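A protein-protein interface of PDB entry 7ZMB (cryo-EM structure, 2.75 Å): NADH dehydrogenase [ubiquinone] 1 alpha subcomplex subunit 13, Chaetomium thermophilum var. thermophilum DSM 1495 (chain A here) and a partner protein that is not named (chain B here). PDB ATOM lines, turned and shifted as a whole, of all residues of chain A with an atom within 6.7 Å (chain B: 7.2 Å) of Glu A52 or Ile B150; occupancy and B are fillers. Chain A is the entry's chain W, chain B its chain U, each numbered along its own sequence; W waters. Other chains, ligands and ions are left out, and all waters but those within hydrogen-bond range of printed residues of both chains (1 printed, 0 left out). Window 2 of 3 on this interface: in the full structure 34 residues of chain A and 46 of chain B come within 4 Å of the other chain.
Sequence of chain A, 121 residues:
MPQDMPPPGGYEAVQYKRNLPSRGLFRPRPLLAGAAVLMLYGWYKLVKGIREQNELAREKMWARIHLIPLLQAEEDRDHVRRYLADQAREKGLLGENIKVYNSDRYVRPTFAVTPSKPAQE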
ATOM      1  N   LYS A  45      -7.387  -5.569  13.991  1.00  0.00           N
ATOM      2  CA  LYS A  45      -8.820  -5.365  13.800  1.00  0.00           C
ATOM      3  C   LYS A  45      -9.170  -3.896  13.643  1.00  0.00           C
ATOM      4  O   LYS A  45     -10.124  -3.559  12.937  1.00  0.00           O
ATOM      5  CB  LYS A  45      -9.605  -5.950  14.971  1.00  0.00           C
ATOM      6  CG  LYS A  45      -9.463  -7.429  15.150  1.00  0.00           C
ATOM      7  CD  LYS A  45     -10.112  -8.136  13.984  1.00  0.00           C
ATOM      8  CE  LYS A  45     -10.070  -9.619  14.143  1.00  0.00           C
ATOM      9  NZ  LYS A  45     -10.672 -10.283  12.968  1.00  0.00           N
ATOM     10  N   LEU A  46      -8.438  -3.011  14.318  1.00  0.00           N
ATOM     11  CA  LEU A  46      -8.740  -1.595  14.219  1.00  0.00           C
ATOM     12  C   LEU A  46      -8.446  -1.071  12.819  1.00  0.00           C
ATOM     13  O   LEU A  46      -9.196  -0.244  12.292  1.00  0.00           O
ATOM     14  CB  LEU A  46      -7.945  -0.822  15.267  1.00  0.00           C
ATOM     15  CG  LEU A  46      -8.397   0.629  15.449  1.00  0.00           C
ATOM     16  CD1 LEU A  46      -9.765   0.675  16.135  1.00  0.00           C
ATOM     17  CD2 LEU A  46      -7.372   1.455  16.191  1.00  0.00           C
ATOM     18  N   VAL A  47      -7.357  -1.536  12.202  1.00  0.00           N
ATOM     19  CA  VAL A  47      -7.043  -1.139  10.833  1.00  0.00           C
ATOM     20  C   VAL A  47      -8.135  -1.608   9.880  1.00  0.00           C
ATOM     21  O   VAL A  47      -8.569  -0.859   9.003  1.00  0.00           O
ATOM     22  CB  VAL A  47      -5.657  -1.673  10.422  1.00  0.00           C
ATOM     23  CG1 VAL A  47      -5.515  -1.710   8.913  1.00  0.00           C
ATOM     24  CG2 VAL A  47      -4.566  -0.827  11.019  1.00  0.00           C
ATOM     25  N   LYS A  48      -8.605  -2.848  10.043  1.00  0.00           N
ATOM     26  CA  LYS A  48      -9.730  -3.329   9.245  1.00  0.00           C
ATOM     27  C   LYS A  48     -10.982  -2.496   9.478  1.00  0.00           C
ATOM     28  O   LYS A  48     -11.684  -2.137   8.529  1.00  0.00           O
ATOM     29  CB  LYS A  48     -10.017  -4.797   9.568  1.00  0.00           C
ATOM     30  CG  LYS A  48      -8.893  -5.787   9.296  1.00  0.00           C
ATOM     31  CD  LYS A  48      -8.649  -6.011   7.811  1.00  0.00           C
ATOM     32  CE  LYS A  48      -7.565  -5.114   7.242  1.00  0.00           C
ATOM     33  NZ  LYS A  48      -7.283  -5.437   5.816  1.00  0.00           N
ATOM     34  N   GLY A  49     -11.301  -2.203  10.740  1.00  0.00           N
ATOM     35  CA  GLY A  49     -12.535  -1.470  11.071  1.00  0.00           C
ATOM     36  C   GLY A  49     -12.589  -0.084  10.473  1.00  0.00           C
ATOM     37  O   GLY A  49     -13.623   0.262   9.889  1.00  0.00           O
ATOM     38  N   ILE A  50     -11.545   0.709  10.711  1.00  0.00           N
ATOM     39  CA  ILE A  50     -11.518   2.119  10.235  1.00  0.00           C
ATOM     40  C   ILE A  50     -11.457   2.150   8.710  1.00  0.00           C
ATOM     41  O   ILE A  50     -12.104   3.019   8.109  1.00  0.00           O
ATOM     42  CB  ILE A  50     -10.400   2.920  10.924  1.00  0.00           C
ATOM     43  CG1 ILE A  50     -10.503   2.804  12.447  1.00  0.00           C
ATOM     44  CG2 ILE A  50     -10.424   4.371  10.475  1.00  0.00           C
ATOM     45  CD1 ILE A  50      -9.425   3.539  13.203  1.00  0.00           C
ATOM     46  N   ARG A  51     -10.724   1.219   8.109  1.00  0.00           N
ATOM     47  CA  ARG A  51     -10.700   1.183   6.633  1.00  0.00           C
ATOM     48  C   ARG A  51     -12.121   0.939   6.107  1.00  0.00           C
ATOM     49  O   ARG A  51     -12.509   1.638   5.161  1.00  0.00           O
ATOM     50  CB  ARG A  51      -9.609   0.238   6.137  1.00  0.00           C
ATOM     51  CG  ARG A  51      -8.220   0.860   6.159  1.00  0.00           C
ATOM     52  CD  ARG A  51      -7.142  -0.105   5.720  1.00  0.00           C
ATOM     53  NE  ARG A  51      -5.791   0.430   5.791  1.00  0.00           N
ATOM     54  CZ  ARG A  51      -4.712  -0.226   5.382  1.00  0.00           C
ATOM     55  NH1 ARG A  51      -3.517   0.328   5.486  1.00  0.00           N
ATOM     56  NH2 ARG A  51      -4.835  -1.435   4.866  1.00  0.00           N
ATOM     57  N   GLU A  52     -12.876   0.032   6.729  1.00  0.00           N
ATOM     58  CA  GLU A  52     -14.275  -0.261   6.318  1.00  0.00           C
ATOM     59  C   GLU A  52     -15.190   0.934   6.589  1.00  0.00           C
ATOM     60  O   GLU A  52     -16.031   1.215   5.730  1.00  0.00           O
ATOM     61  CB  GLU A  52     -14.782  -1.523   7.014  1.00  0.00           C
ATOM     62  CG  GLU A  52     -15.804  -2.279   6.192  1.00  0.00           C
ATOM     63  CD  GLU A  52     -16.839  -3.045   6.990  1.00  0.00           C
ATOM     64  OE1 GLU A  52     -17.268  -2.524   8.031  1.00  0.00           O
ATOM     65  OE2 GLU A  52     -17.207  -4.159   6.567  1.00  0.00           O
ATOM     66  N   GLN A  53     -15.036   1.595   7.741  1.00  0.00           N
ATOM     67  CA  GLN A  53     -15.912   2.738   8.123  1.00  0.00           C
ATOM     68  C   GLN A  53     -15.686   3.924   7.180  1.00  0.00           C
ATOM     69  O   GLN A  53     -16.655   4.624   6.891  1.00  0.00           O
ATOM     70  CB  GLN A  53     -15.860   3.054   9.619  1.00  0.00           C
ATOM     71  CG  GLN A  53     -14.707   3.951  10.031  1.00  0.00           C
ATOM     72  CD  GLN A  53     -14.810   4.296  11.494  1.00  0.00           C
ATOM     73  OE1 GLN A  53     -15.532   3.655  12.252  1.00  0.00           O
ATOM     74  NE2 GLN A  53     -14.093   5.329  11.896  1.00  0.00           N
ATOM     75  N   ASN A  54     -14.451   4.144   6.743  1.00  0.00           N
ATOM     76  CA  ASN A  54     -14.158   5.246   5.799  1.00  0.00           C
ATOM     77  C   ASN A  54     -14.825   4.913   4.468  1.00  0.00           C
ATOM     78  O   ASN A  54     -15.327   5.850   3.837  1.00  0.00           O
ATOM     79  CB  ASN A  54     -12.660   5.577   5.730  1.00  0.00           C
ATOM     80  CG  ASN A  54     -12.111   6.186   7.003  1.00  0.00           C
ATOM     81  OD1 ASN A  54     -12.830   6.355   7.985  1.00  0.00           O
ATOM     82  ND2 ASN A  54     -10.832   6.518   6.997  1.00  0.00           N
ATOM     83  N   GLU A  55     -14.798   3.642   4.052  1.00  0.00           N
ATOM     84  CA  GLU A  55     -15.525   3.200   2.837  1.00  0.00           C
ATOM     85  C   GLU A  55     -17.041   3.322   3.030  1.00  0.00           C
ATOM     86  O   GLU A  55     -17.720   3.699   2.068  1.00  0.00           O
ATOM     87  CB  GLU A  55     -15.061   1.794   2.468  1.00  0.00           C
ATOM     88  CG  GLU A  55     -13.650   1.789   1.931  1.00  0.00           C
ATOM     89  CD  GLU A  55     -13.384   2.983   1.034  1.00  0.00           C
ATOM     90  OE1 GLU A  55     -12.459   3.759   1.341  1.00  0.00           O
ATOM     91  OE2 GLU A  55     -14.103   3.130   0.026  1.00  0.00           O
ATOM     92  N   LEU A  56     -17.548   3.001   4.219  1.00  0.00           N
ATOM     93  CA  LEU A  56     -18.991   3.154   4.529  1.00  0.00           C
ATOM     94  C   LEU A  56     -19.334   4.637   4.440  1.00  0.00           C
ATOM     95  O   LEU A  56     -20.422   4.954   3.944  1.00  0.00           O
ATOM     96  CB  LEU A  56     -19.245   2.612   5.939  1.00  0.00           C
ATOM     97  CG  LEU A  56     -19.339   1.096   6.063  1.00  0.00           C
ATOM     98  CD1 LEU A  56     -19.698   0.710   7.487  1.00  0.00           C
ATOM     99  CD2 LEU A  56     -20.364   0.542   5.091  1.00  0.00           C
ATOM    100  N   ALA A  57     -18.429   5.499   4.910  1.00  0.00           N
ATOM    101  CA  ALA A  57     -18.616   6.963   4.832  1.00  0.00           C
ATOM    102  C   ALA A  57     -18.657   7.438   3.375  1.00  0.00           C
ATOM    103  O   ALA A  57     -19.457   8.333   3.091  1.00  0.00           O
ATOM    104  CB  ALA A  57     -17.548   7.649   5.637  1.00  0.00           C
ATOM    105  N   TRP B 110     -25.483  -0.073   5.448  1.00  0.00           N
ATOM    106  CA  TRP B 110     -24.815  -1.340   5.839  1.00  0.00           C
ATOM    107  C   TRP B 110     -25.751  -2.203   6.688  1.00  0.00           C
ATOM    108  O   TRP B 110     -25.465  -3.393   6.834  1.00  0.00           O
ATOM    109  CB  TRP B 110     -23.476  -1.071   6.532  1.00  0.00           C
ATOM    110  CG  TRP B 110     -23.544  -0.304   7.815  1.00  0.00           C
ATOM    111  CD1 TRP B 110     -23.632  -0.814   9.077  1.00  0.00           C
ATOM    112  CD2 TRP B 110     -23.476   1.124   7.963  1.00  0.00           C
ATOM    113  NE1 TRP B 110     -23.641   0.198   9.997  1.00  0.00           N
ATOM    114  CE2 TRP B 110     -23.542   1.397   9.344  1.00  0.00           C
ATOM    115  CE3 TRP B 110     -23.366   2.191   7.067  1.00  0.00           C
ATOM    116  CZ2 TRP B 110     -23.509   2.696   9.843  1.00  0.00           C
ATOM    117  CZ3 TRP B 110     -23.332   3.472   7.563  1.00  0.00           C
ATOM    118  CH2 TRP B 110     -23.406   3.720   8.932  1.00  0.00           C
ATOM    119  N   VAL B 143     -17.385  -2.078  -0.436  1.00  0.00           N
ATOM    120  CA  VAL B 143     -18.075  -2.276   0.877  1.00  0.00           C
ATOM    121  C   VAL B 143     -19.553  -2.670   0.704  1.00  0.00           C
ATOM    122  O   VAL B 143     -20.090  -3.323   1.601  1.00  0.00           O
ATOM    123  CB  VAL B 143     -17.862  -1.080   1.827  1.00  0.00           C
ATOM    124  CG1 VAL B 143     -18.827   0.060   1.539  1.00  0.00           C
ATOM    125  CG2 VAL B 143     -17.924  -1.494   3.288  1.00  0.00           C
ATOM    126  N   ARG B 146     -19.551  -6.433   0.046  1.00  0.00           N
ATOM    127  CA  ARG B 146     -18.851  -7.305   1.027  1.00  0.00           C
ATOM    128  C   ARG B 146     -19.875  -8.210   1.703  1.00  0.00           C
ATOM    129  O   ARG B 146     -20.933  -7.704   2.093  1.00  0.00           O
ATOM    130  CB  ARG B 146     -18.047  -6.518   2.062  1.00  0.00           C
ATOM    131  CG  ARG B 146     -16.728  -5.973   1.549  1.00  0.00           C
ATOM    132  CD  ARG B 146     -15.941  -5.162   2.553  1.00  0.00           C
ATOM    133  NE  ARG B 146     -15.009  -4.318   1.823  1.00  0.00           N
ATOM    134  CZ  ARG B 146     -14.199  -3.430   2.376  1.00  0.00           C
ATOM    135  NH1 ARG B 146     -13.398  -2.710   1.613  1.00  0.00           N
ATOM    136  NH2 ARG B 146     -14.185  -3.269   3.685  1.00  0.00           N
ATOM    137  N   ARG B 148     -19.568  -9.767   4.568  1.00  0.00           N
ATOM    138  CA  ARG B 148     -19.651  -9.534   6.021  1.00  0.00           C
ATOM    139  C   ARG B 148     -19.624  -8.028   6.282  1.00  0.00           C
ATOM    140  O   ARG B 148     -18.689  -7.368   5.803  1.00  0.00           O
ATOM    141  CB  ARG B 148     -18.517 -10.288   6.710  1.00  0.00           C
ATOM    142  CG  ARG B 148     -18.730 -11.791   6.791  1.00  0.00           C
ATOM    143  CD  ARG B 148     -18.004 -12.356   7.995  1.00  0.00           C
ATOM    144  NE  ARG B 148     -18.339 -11.599   9.193  1.00  0.00           N
ATOM    145  CZ  ARG B 148     -17.860 -11.853  10.404  1.00  0.00           C
ATOM    146  NH1 ARG B 148     -18.226 -11.106  11.431  1.00  0.00           N
ATOM    147  NH2 ARG B 148     -17.018 -12.856  10.584  1.00  0.00           N
ATOM    148  N   GLN B 149     -20.637  -7.510   6.976  1.00  0.00           N
ATOM    149  CA  GLN B 149     -20.604  -6.078   7.347  1.00  0.00           C
ATOM    150  C   GLN B 149     -20.188  -5.975   8.813  1.00  0.00           C
ATOM    151  O   GLN B 149     -20.937  -6.470   9.654  1.00  0.00           O
ATOM    152  CB  GLN B 149     -21.896  -5.348   6.984  1.00  0.00           C
ATOM    153  CG  GLN B 149     -22.175  -5.299   5.491  1.00  0.00           C
ATOM    154  CD  GLN B 149     -21.123  -4.589   4.674  1.00  0.00           C
ATOM    155  OE1 GLN B 149     -20.565  -3.570   5.072  1.00  0.00           O
ATOM    156  NE2 GLN B 149     -20.871  -5.114   3.489  1.00  0.00           N
ATOM    157  N   ILE B 150     -19.079  -5.296   9.107  1.00  0.00           N
ATOM    158  CA  ILE B 150     -18.558  -5.264  10.507  1.00  0.00           C
ATOM    159  C   ILE B 150     -19.402  -4.333  11.384  1.00  0.00           C
ATOM    160  O   ILE B 150     -19.460  -4.588  12.605  1.00  0.00           O
ATOM    161  CB  ILE B 150     -17.108  -4.732  10.468  1.00  0.00           C
ATOM    162  CG1 ILE B 150     -16.176  -5.612   9.631  1.00  0.00           C
ATOM    163  CG2 ILE B 150     -16.547  -4.499  11.863  1.00  0.00           C
ATOM    164  CD1 ILE B 150     -14.779  -5.053   9.501  1.00  0.00           C
ATOM    165  N   PHE B 151     -20.119  -3.373  10.799  1.00  0.00           N
ATOM    166  CA  PHE B 151     -20.853  -2.396  11.644  1.00  0.00           C
ATOM    167  C   PHE B 151     -22.343  -2.745  11.700  1.00  0.00           C
ATOM    168  O   PHE B 151     -23.096  -2.015  12.363  1.00  0.00           O
ATOM    169  CB  PHE B 151     -20.468  -0.963  11.268  1.00  0.00           C
ATOM    170  CG  PHE B 151     -19.029  -0.632  11.564  1.00  0.00           C
ATOM    171  CD1 PHE B 151     -18.626  -0.319  12.852  1.00  0.00           C
ATOM    172  CD2 PHE B 151     -18.074  -0.656  10.563  1.00  0.00           C
ATOM    173  CE1 PHE B 151     -17.299  -0.026  13.130  1.00  0.00           C
ATOM    174  CE2 PHE B 151     -16.749  -0.367  10.843  1.00  0.00           C
ATOM    175  CZ  PHE B 151     -16.365  -0.051  12.123  1.00  0.00           C
ATOM    176  N   ALA B 152     -22.736  -3.852  11.067  1.00  0.00           N
ATOM    177  CA  ALA B 152     -24.151  -4.296  11.069  1.00  0.00           C
ATOM    178  C   ALA B 152     -24.472  -4.974  12.402  1.00  0.00           C
ATOM    179  O   ALA B 152     -23.693  -5.847  12.810  1.00  0.00           O
ATOM    180  CB  ALA B 152     -24.400  -5.239   9.930  1.00  0.00           C
ATOM    181  N   HIS B 153     -25.574  -4.580  13.044  1.00  0.00           N
ATOM    182  CA  HIS B 153     -25.970  -5.225  14.326  1.00  0.00           C
ATOM    183  C   HIS B 153     -26.380  -6.678  14.103  1.00  0.00           C
ATOM    184  O   HIS B 153     -26.005  -7.517  14.922  1.00  0.00           O
ATOM    185  CB  HIS B 153     -26.973  -4.382  15.112  1.00  0.00           C
ATOM    186  CG  HIS B 153     -28.116  -3.840  14.336  1.00  0.00           C
ATOM    187  ND1 HIS B 153     -29.120  -4.640  13.848  1.00  0.00           N
ATOM    188  CD2 HIS B 153     -28.444  -2.572  14.020  1.00  0.00           C
ATOM    189  CE1 HIS B 153     -30.008  -3.894  13.231  1.00  0.00           C
ATOM    190  NE2 HIS B 153     -29.614  -2.621  13.322  1.00  0.00           N
ATOM    191  N   ILE B 156     -24.973 -10.408   8.382  1.00  0.00           N
ATOM    192  CA  ILE B 156     -25.546 -10.719   7.045  1.00  0.00           C
ATOM    193  C   ILE B 156     -25.633 -12.239   6.973  1.00  0.00           C
ATOM    194  O   ILE B 156     -24.657 -12.906   7.332  1.00  0.00           O
ATOM    195  CB  ILE B 156     -24.704 -10.103   5.900  1.00  0.00           C
ATOM    196  CG1 ILE B 156     -24.993  -8.613   5.720  1.00  0.00           C
ATOM    197  CG2 ILE B 156     -24.919 -10.855   4.597  1.00  0.00           C
ATOM    198  CD1 ILE B 156     -24.474  -7.751   6.833  1.00  0.00           C
HETATM  199  O   HOH W   1     -19.967  -2.596   7.986  1.00  0.00           O
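The backbone NH of Ile B150 sits at hydrogen-bond distance from the side-chain carboxylate of Glu A52 (3.4 Å).
The indole nitrogen (NE1) of Trp B110 sits at hydrogen-bond distance from the backbone carbonyl oxygen (O) of Phe B151 (3.3 Å). O of Val B143 is in hydrogen-bond range of NE2 of Gln B149, at 2.7 Å. The backbone carbonyl oxygen (O) of Arg B146 lies within hydrogen-bond range of the side-chain amide nitrogen (NE2) of Gln B149, 2.9 Å away.
CE2 of Phe B151 touches O of Gly A49 (3.3 Å). Glu A52 touches Val B143 (CG to CG2, 3.7 Å). CG of Glu A52 touches NH2 of Arg B146 (3.1 Å). Arg B148 touches Glu A52. Glu A52 touches Gln B149 (OE2 to OE1, 3.7 Å). CD2 of Phe B151 touches OE1 of Glu A52, at 3.2 Å. Gln A53 touches Phe B151 (CB to CE2, 3.7 Å). O of Glu A55 touches CG1 of Val B143 (3.8 Å). Val B143 touches Leu A56. Phe B151 touches Leu A56.
Glu A52 touches just these residues of chain B: Val B143, Arg B146, Arg B148, Gln B149, Ile B150 and Phe B151. Of the printed residues of chain B, Leu A56 touches Trp B110, Val B143 and Phe B151. Ala A57 touches none of the printed residues of chain B. Printed residues of chain A within 4 Å of Arg B148: Glu A52 (3.6 Å). Of chain A, only Glu A52 comes within 4 Å of Ile B150. Printed residues of chain A within 4 Å of Phe B151: Gly A49 (3.3 Å), Glu A52 (3.2 Å), Gln A53 (3.7 Å) and Leu A56 (3.7 Å). The nearest printed residue of chain B that does not touch Gly A49 is Ile B150 (4.5 Å).
Of the 10 printed residues of chain B, 7 touch a printed residue of chain A. Printed residues of chain A that touch a printed residue of chain B: Gly A49, Glu A52, Gln A53, Glu A55 and Leu A56.
Water W1 lies within hydrogen-bond range of the side-chain carboxylate of Glu A52, the backbone NH of Phe B151, the backbone NH of Ile B150 and the side-chain amide oxygen of Gln B149.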
